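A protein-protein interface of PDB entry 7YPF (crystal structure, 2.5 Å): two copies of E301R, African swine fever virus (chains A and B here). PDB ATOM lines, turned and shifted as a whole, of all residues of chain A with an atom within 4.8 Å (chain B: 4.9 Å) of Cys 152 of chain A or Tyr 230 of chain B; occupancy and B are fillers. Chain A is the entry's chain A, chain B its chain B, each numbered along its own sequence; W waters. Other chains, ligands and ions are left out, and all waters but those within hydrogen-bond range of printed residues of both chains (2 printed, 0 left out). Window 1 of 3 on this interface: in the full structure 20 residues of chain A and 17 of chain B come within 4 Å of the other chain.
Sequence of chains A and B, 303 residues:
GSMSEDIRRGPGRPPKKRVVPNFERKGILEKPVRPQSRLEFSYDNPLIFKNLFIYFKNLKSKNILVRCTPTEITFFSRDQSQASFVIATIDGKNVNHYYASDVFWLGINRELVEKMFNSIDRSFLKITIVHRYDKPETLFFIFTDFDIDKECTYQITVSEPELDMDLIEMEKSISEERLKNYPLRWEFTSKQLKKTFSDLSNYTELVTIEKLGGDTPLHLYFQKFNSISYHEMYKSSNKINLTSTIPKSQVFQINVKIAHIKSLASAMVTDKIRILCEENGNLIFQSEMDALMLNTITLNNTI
OH of Tyr 230 of chain B is in hydrogen-bond range of SG of Cys 152 of chain A (3.3 Å).
The backbone carbonyl oxygen (O) of His 231 of chain B is in hydrogen-bond range of the backbone NH (N) of Thr 153 of chain A (2.7 Å).
O of Phe 143 of chain A sits at hydrogen-bond distance from N of Cys 152 of chain A (2.8 Å).
N of Tyr 154 of chain A sits at hydrogen-bond distance from O of Phe 141 of chain A (2.7 Å).
N of Phe 222 of chain B is in hydrogen-bond range of O of Tyr 230 of chain B.
The backbone carbonyl oxygen of Leu 220 of chain B is in hydrogen-bond range of the backbone NH of Glu 232 of chain B, at 2.6 Å.
The side-chain hydroxyl (OH) of Tyr 230 of chain B sits at hydrogen-bond distance from the side-chain carboxylate (OE1) of Glu 232 of chain B, 2.7 Å away.
Among the printed residues, merely in contact across the chains: Lys 150 of chain A with Glu 232 of chain B (3.7 Å), Glu 151 of chain A with His 231 of chain B (3.5 Å), Glu 151 of chain A with Glu 232 of chain B (3.4 Å), Cys 152 of chain A with His 231 of chain B (3.5 Å), Cys 152 of chain A with Glu 232 of chain B (3.8 Å), Thr 153 of chain A with Ser 229 of chain B (3.9 Å), Thr 153 of chain A with Tyr 230 of chain B (3.4 Å), Tyr 154 of chain A with Ile 228 of chain B (3.9 Å), Tyr 154 of chain A with Ser 229 of chain B (3.5 Å) and Tyr 154 of chain A with Tyr 230 of chain B (3.4 Å).
Phe 124 of chain A touches none of the printed residues of chain B.
Phe 143 of chain A touches none of the printed residues of chain B.
Of the printed residues of chain B, Tyr 154 of chain A touches Ile 228, Ser 229 and Tyr 230.
Of the printed residues of chain A, Ile 228 of chain B touches Tyr 154 (3.9 Å).
Printed residues of chain A within 4 Å of Ser 229 of chain B: Thr 153 and Tyr 154.
Tyr 230 of chain B touches just these residues of chain A: Cys 152 (3.3 Å), Thr 153 (3.4 Å) and Tyr 154 (3.4 Å).
Printed residues of chain A within 4 Å of His 231 of chain B: Glu 151 (3.5 Å), Cys 152 (3.5 Å) and Thr 153 (2.7 Å).
Printed residues of chain A within 4 Å of Glu 232 of chain B: Lys 150, Glu 151 and Cys 152.
Of the 9 printed residues of chain A, 5 touch a printed residue of chain B.
Hydrophobic or aromatic side chains of chain A that line the printed part of chain B: Tyr 154.
Among the printed residues, 12 pairs touch across the chains.
No position is printed for both chains.
Of the 12 pairs that touch across the chains among the printed residues, none has its exchanged pair printed and touching as well.
Water W1 lies within hydrogen-bond range of the side-chain hydroxyl of Thr 153 of chain A, the backbone carbonyl oxygen of His 231 of chain B and the backbone carbonyl oxygen of Glu 151 of chain A.
Water W2 bridges the side-chain hydroxyl of Tyr 154 of chain A and the backbone carbonyl oxygen of Asp 199 of chain B.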
ATOM      1  N   PHE A 124     -30.825 -34.539   8.233  1.00  0.00           N
ATOM      2  CA  PHE A 124     -30.012 -33.347   8.025  1.00  0.00           C
ATOM      3  C   PHE A 124     -29.559 -33.300   6.572  1.00  0.00           C
ATOM      4  O   PHE A 124     -28.965 -34.260   6.072  1.00  0.00           O
ATOM      5  CB  PHE A 124     -28.788 -33.332   8.945  1.00  0.00           C
ATOM      6  CG  PHE A 124     -29.119 -33.226  10.407  1.00  0.00           C
ATOM      7  CD1 PHE A 124     -30.109 -32.364  10.851  1.00  0.00           C
ATOM      8  CD2 PHE A 124     -28.419 -33.976  11.341  1.00  0.00           C
ATOM      9  CE1 PHE A 124     -30.409 -32.262  12.201  1.00  0.00           C
ATOM     10  CE2 PHE A 124     -28.709 -33.878  12.690  1.00  0.00           C
ATOM     11  CZ  PHE A 124     -29.706 -33.020  13.122  1.00  0.00           C
ATOM     12  N   PHE A 141     -20.549 -26.330  14.757  1.00  0.00           N
ATOM     13  CA  PHE A 141     -21.106 -27.287  13.807  1.00  0.00           C
ATOM     14  C   PHE A 141     -22.620 -27.134  13.818  1.00  0.00           C
ATOM     15  O   PHE A 141     -23.260 -27.362  14.850  1.00  0.00           O
ATOM     16  CB  PHE A 141     -20.713 -28.725  14.160  1.00  0.00           C
ATOM     17  CG  PHE A 141     -19.232 -28.976  14.152  1.00  0.00           C
ATOM     18  CD1 PHE A 141     -18.463 -28.711  15.273  1.00  0.00           C
ATOM     19  CD2 PHE A 141     -18.608 -29.491  13.025  1.00  0.00           C
ATOM     20  CE1 PHE A 141     -17.097 -28.946  15.271  1.00  0.00           C
ATOM     21  CE2 PHE A 141     -17.242 -29.729  13.015  1.00  0.00           C
ATOM     22  CZ  PHE A 141     -16.487 -29.455  14.141  1.00  0.00           C
ATOM     23  N   ILE A 142     -23.190 -26.749  12.678  1.00  0.00           N
ATOM     24  CA  ILE A 142     -24.626 -26.536  12.547  1.00  0.00           C
ATOM     25  C   ILE A 142     -25.196 -27.573  11.588  1.00  0.00           C
ATOM     26  O   ILE A 142     -24.731 -27.699  10.448  1.00  0.00           O
ATOM     27  CB  ILE A 142     -24.948 -25.112  12.066  1.00  0.00           C
ATOM     28  CG1 ILE A 142     -24.368 -24.079  13.033  1.00  0.00           C
ATOM     29  CG2 ILE A 142     -26.452 -24.927  11.934  1.00  0.00           C
ATOM     30  CD1 ILE A 142     -23.523 -23.025  12.359  1.00  0.00           C
ATOM     31  N   PHE A 143     -26.205 -28.306  12.050  1.00  0.00           N
ATOM     32  CA  PHE A 143     -26.929 -29.274  11.240  1.00  0.00           C
ATOM     33  C   PHE A 143     -28.355 -28.774  11.054  1.00  0.00           C
ATOM     34  O   PHE A 143     -29.003 -28.369  12.025  1.00  0.00           O
ATOM     35  CB  PHE A 143     -26.924 -30.654  11.899  1.00  0.00           C
ATOM     36  CG  PHE A 143     -25.546 -31.204  12.137  1.00  0.00           C
ATOM     37  CD1 PHE A 143     -24.721 -31.528  11.074  1.00  0.00           C
ATOM     38  CD2 PHE A 143     -25.072 -31.386  13.427  1.00  0.00           C
ATOM     39  CE1 PHE A 143     -23.453 -32.033  11.291  1.00  0.00           C
ATOM     40  CE2 PHE A 143     -23.803 -31.889  13.650  1.00  0.00           C
ATOM     41  CZ  PHE A 143     -22.992 -32.212  12.581  1.00  0.00           C
ATOM     42  N   LYS A 150     -35.356 -26.993  11.575  1.00  0.00           N
ATOM     43  CA  LYS A 150     -34.691 -27.208  12.852  1.00  0.00           C
ATOM     44  C   LYS A 150     -33.191 -27.044  12.653  1.00  0.00           C
ATOM     45  O   LYS A 150     -32.588 -27.751  11.839  1.00  0.00           O
ATOM     46  CB  LYS A 150     -35.015 -28.593  13.409  1.00  0.00           C
ATOM     47  CG  LYS A 150     -34.224 -28.960  14.649  1.00  0.00           C
ATOM     48  CD  LYS A 150     -34.660 -30.311  15.186  1.00  0.00           C
ATOM     49  CE  LYS A 150     -34.126 -31.445  14.329  1.00  0.00           C
ATOM     50  NZ  LYS A 150     -34.078 -32.732  15.077  1.00  0.00           N
ATOM     51  N   GLU A 151     -32.593 -26.111  13.390  1.00  0.00           N
ATOM     52  CA  GLU A 151     -31.154 -25.884  13.366  1.00  0.00           C
ATOM     53  C   GLU A 151     -30.547 -26.429  14.651  1.00  0.00           C
ATOM     54  O   GLU A 151     -30.942 -26.024  15.750  1.00  0.00           O
ATOM     55  CB  GLU A 151     -30.830 -24.399  13.203  1.00  0.00           C
ATOM     56  CG  GLU A 151     -30.348 -24.030  11.811  1.00  0.00           C
ATOM     57  CD  GLU A 151     -29.885 -22.592  11.714  1.00  0.00           C
ATOM     58  OE1 GLU A 151     -29.290 -22.092  12.690  1.00  0.00           O
ATOM     59  OE2 GLU A 151     -30.104 -21.965  10.656  1.00  0.00           O
ATOM     60  N   CYS A 152     -29.591 -27.345  14.509  1.00  0.00           N
ATOM     61  CA  CYS A 152     -28.885 -27.951  15.633  1.00  0.00           C
ATOM     62  C   CYS A 152     -27.454 -27.432  15.619  1.00  0.00           C
ATOM     63  O   CYS A 152     -26.669 -27.782  14.729  1.00  0.00           O
ATOM     64  CB  CYS A 152     -28.924 -29.475  15.551  1.00  0.00           C
ATOM     65  SG  CYS A 152     -30.592 -30.160  15.447  1.00  0.00           S
ATOM     66  N   THR A 153     -27.116 -26.601  16.599  1.00  0.00           N
ATOM     67  CA  THR A 153     -25.814 -25.952  16.671  1.00  0.00           C
ATOM     68  C   THR A 153     -24.994 -26.562  17.799  1.00  0.00           C
ATOM     69  O   THR A 153     -25.450 -26.616  18.948  1.00  0.00           O
ATOM     70  CB  THR A 153     -25.960 -24.446  16.888  1.00  0.00           C
ATOM     71  OG1 THR A 153     -26.745 -23.885  15.830  1.00  0.00           O
ATOM     72  CG2 THR A 153     -24.594 -23.778  16.911  1.00  0.00           C
ATOM     73  N   TYR A 154     -23.790 -27.016  17.466  1.00  0.00           N
ATOM     74  CA  TYR A 154     -22.829 -27.512  18.439  1.00  0.00           C
ATOM     75  C   TYR A 154     -21.722 -26.483  18.607  1.00  0.00           C
ATOM     76  O   TYR A 154     -21.138 -26.027  17.618  1.00  0.00           O
ATOM     77  CB  TYR A 154     -22.229 -28.848  17.996  1.00  0.00           C
ATOM     78  CG  TYR A 154     -23.177 -30.022  18.061  1.00  0.00           C
ATOM     79  CD1 TYR A 154     -24.125 -30.230  17.069  1.00  0.00           C
ATOM     80  CD2 TYR A 154     -23.112 -30.933  19.108  1.00  0.00           C
ATOM     81  CE1 TYR A 154     -24.989 -31.305  17.122  1.00  0.00           C
ATOM     82  CE2 TYR A 154     -23.975 -32.012  19.171  1.00  0.00           C
ATOM     83  CZ  TYR A 154     -24.910 -32.193  18.174  1.00  0.00           C
ATOM     84  OH  TYR A 154     -25.769 -33.266  18.231  1.00  0.00           O
ATOM     85  N   ASP B 199     -30.186 -37.634  20.873  1.00  0.00           N
ATOM     86  CA  ASP B 199     -29.006 -36.786  20.742  1.00  0.00           C
ATOM     87  C   ASP B 199     -28.690 -36.083  22.056  1.00  0.00           C
ATOM     88  O   ASP B 199     -27.534 -36.051  22.493  1.00  0.00           O
ATOM     89  CB  ASP B 199     -29.216 -35.769  19.618  1.00  0.00           C
ATOM     90  CG  ASP B 199     -29.309 -36.420  18.250  1.00  0.00           C
ATOM     91  OD1 ASP B 199     -29.264 -37.668  18.175  1.00  0.00           O
ATOM     92  OD2 ASP B 199     -29.425 -35.682  17.249  1.00  0.00           O
ATOM     93  N   LEU B 200     -29.701 -35.565  22.720  1.00  0.00           N
ATOM     94  CA  LEU B 200     -29.504 -34.912  23.968  1.00  0.00           C
ATOM     95  C   LEU B 200     -28.932 -35.843  25.001  1.00  0.00           C
ATOM     96  O   LEU B 200     -28.070 -35.451  25.717  1.00  0.00           O
ATOM     97  CB  LEU B 200     -30.806 -34.317  24.499  1.00  0.00           C
ATOM     98  CG  LEU B 200     -31.335 -33.042  23.892  1.00  0.00           C
ATOM     99  CD1 LEU B 200     -32.764 -32.701  24.221  1.00  0.00           C
ATOM    100  CD2 LEU B 200     -30.395 -31.899  24.026  1.00  0.00           C
ATOM    101  N   LEU B 220     -34.130 -25.207  22.550  1.00  0.00           N
ATOM    102  CA  LEU B 220     -33.718 -26.308  23.414  1.00  0.00           C
ATOM    103  C   LEU B 220     -32.199 -26.309  23.481  1.00  0.00           C
ATOM    104  O   LEU B 220     -31.534 -26.310  22.439  1.00  0.00           O
ATOM    105  CB  LEU B 220     -34.220 -27.656  22.887  1.00  0.00           C
ATOM    106  CG  LEU B 220     -35.618 -28.157  23.263  1.00  0.00           C
ATOM    107  CD1 LEU B 220     -36.703 -27.172  22.858  1.00  0.00           C
ATOM    108  CD2 LEU B 220     -35.871 -29.517  22.633  1.00  0.00           C
ATOM    109  N   TYR B 221     -31.644 -26.323  24.694  1.00  0.00           N
ATOM    110  CA  TYR B 221     -30.195 -26.230  24.800  1.00  0.00           C
ATOM    111  C   TYR B 221     -29.704 -26.725  26.154  1.00  0.00           C
ATOM    112  O   TYR B 221     -30.469 -26.864  27.112  1.00  0.00           O
ATOM    113  CB  TYR B 221     -29.708 -24.792  24.563  1.00  0.00           C
ATOM    114  CG  TYR B 221     -30.201 -23.781  25.575  1.00  0.00           C
ATOM    115  CD1 TYR B 221     -31.447 -23.184  25.441  1.00  0.00           C
ATOM    116  CD2 TYR B 221     -29.413 -23.414  26.659  1.00  0.00           C
ATOM    117  CE1 TYR B 221     -31.899 -22.255  26.361  1.00  0.00           C
ATOM    118  CE2 TYR B 221     -29.856 -22.488  27.586  1.00  0.00           C
ATOM    119  CZ  TYR B 221     -31.099 -21.910  27.432  1.00  0.00           C
ATOM    120  OH  TYR B 221     -31.546 -20.986  28.349  1.00  0.00           O
ATOM    121  N   PHE B 222     -28.400 -26.998  26.197  1.00  0.00           N
ATOM    122  CA  PHE B 222     -27.645 -27.196  27.425  1.00  0.00           C
ATOM    123  C   PHE B 222     -26.260 -26.608  27.209  1.00  0.00           C
ATOM    124  O   PHE B 222     -25.799 -26.469  26.073  1.00  0.00           O
ATOM    125  CB  PHE B 222     -27.549 -28.681  27.821  1.00  0.00           C
ATOM    126  CG  PHE B 222     -26.730 -29.517  26.872  1.00  0.00           C
ATOM    127  CD1 PHE B 222     -25.345 -29.552  26.962  1.00  0.00           C
ATOM    128  CD2 PHE B 222     -27.349 -30.275  25.894  1.00  0.00           C
ATOM    129  CE1 PHE B 222     -24.599 -30.314  26.089  1.00  0.00           C
ATOM    130  CE2 PHE B 222     -26.606 -31.045  25.024  1.00  0.00           C
ATOM    131  CZ  PHE B 222     -25.230 -31.060  25.120  1.00  0.00           C
ATOM    132  N   ILE B 228     -18.550 -28.644  25.527  1.00  0.00           N
ATOM    133  CA  ILE B 228     -19.562 -28.692  24.475  1.00  0.00           C
ATOM    134  C   ILE B 228     -20.828 -28.001  24.960  1.00  0.00           C
ATOM    135  O   ILE B 228     -21.319 -28.277  26.058  1.00  0.00           O
ATOM    136  CB  ILE B 228     -19.874 -30.139  24.037  1.00  0.00           C
ATOM    137  CG1 ILE B 228     -21.079 -30.159  23.093  1.00  0.00           C
ATOM    138  CG2 ILE B 228     -20.112 -31.036  25.248  1.00  0.00           C
ATOM    139  CD1 ILE B 228     -21.377 -31.520  22.509  1.00  0.00           C
ATOM    140  N   SER B 229     -21.346 -27.096  24.138  1.00  0.00           N
ATOM    141  CA  SER B 229     -22.695 -26.580  24.285  1.00  0.00           C
ATOM    142  C   SER B 229     -23.495 -26.960  23.048  1.00  0.00           C
ATOM    143  O   SER B 229     -22.949 -27.077  21.947  1.00  0.00           O
ATOM    144  CB  SER B 229     -22.706 -25.058  24.475  1.00  0.00           C
ATOM    145  OG  SER B 229     -21.969 -24.683  25.625  1.00  0.00           O
ATOM    146  N   TYR B 230     -24.796 -27.146  23.234  1.00  0.00           N
ATOM    147  CA  TYR B 230     -25.658 -27.608  22.156  1.00  0.00           C
ATOM    148  C   TYR B 230     -26.950 -26.814  22.190  1.00  0.00           C
ATOM    149  O   TYR B 230     -27.541 -26.636  23.258  1.00  0.00           O
ATOM    150  CB  TYR B 230     -25.950 -29.107  22.278  1.00  0.00           C
ATOM    151  CG  TYR B 230     -26.962 -29.620  21.280  1.00  0.00           C
ATOM    152  CD1 TYR B 230     -26.623 -29.786  19.945  1.00  0.00           C
ATOM    153  CD2 TYR B 230     -28.255 -29.938  21.672  1.00  0.00           C
ATOM    154  CE1 TYR B 230     -27.545 -30.255  19.026  1.00  0.00           C
ATOM    155  CE2 TYR B 230     -29.183 -30.407  20.759  1.00  0.00           C
ATOM    156  CZ  TYR B 230     -28.821 -30.565  19.438  1.00  0.00           C
ATOM    157  OH  TYR B 230     -29.739 -31.031  18.523  1.00  0.00           O
ATOM    158  N   HIS B 231     -27.381 -26.349  21.023  1.00  0.00           N
ATOM    159  CA  HIS B 231     -28.564 -25.508  20.900  1.00  0.00           C
ATOM    160  C   HIS B 231     -29.358 -26.002  19.704  1.00  0.00           C
ATOM    161  O   HIS B 231     -28.832 -26.055  18.588  1.00  0.00           O
ATOM    162  CB  HIS B 231     -28.191 -24.032  20.732  1.00  0.00           C
ATOM    163  CG  HIS B 231     -29.352 -23.154  20.379  1.00  0.00           C
ATOM    164  ND1 HIS B 231     -29.244 -22.090  19.511  1.00  0.00           N
ATOM    165  CD2 HIS B 231     -30.645 -23.181  20.782  1.00  0.00           C
ATOM    166  CE1 HIS B 231     -30.421 -21.501  19.390  1.00  0.00           C
ATOM    167  NE2 HIS B 231     -31.287 -22.144  20.150  1.00  0.00           N
ATOM    168  N   GLU B 232     -30.616 -26.334  19.962  1.00  0.00           N
ATOM    169  CA  GLU B 232     -31.589 -26.797  18.996  1.00  0.00           C
ATOM    170  C   GLU B 232     -32.658 -25.735  18.828  1.00  0.00           C
ATOM    171  O   GLU B 232     -33.326 -25.373  19.740  1.00  0.00           O
ATOM    172  CB  GLU B 232     -32.199 -28.110  19.422  1.00  0.00           C
ATOM    173  CG  GLU B 232     -32.810 -28.880  18.295  1.00  0.00           C
ATOM    174  CD  GLU B 232     -33.268 -30.263  18.652  1.00  0.00           C
ATOM    175  OE1 GLU B 232     -32.440 -31.175  18.635  1.00  0.00           O
ATOM    176  OE2 GLU B 232     -34.470 -30.480  18.914  1.00  0.00           O
HETATM  177  O   HOH W   1     -29.197 -23.984  16.746  1.00  0.00           O
HETATM  178  O   HOH W   2     -25.437 -35.932  19.812  1.00  0.00           O
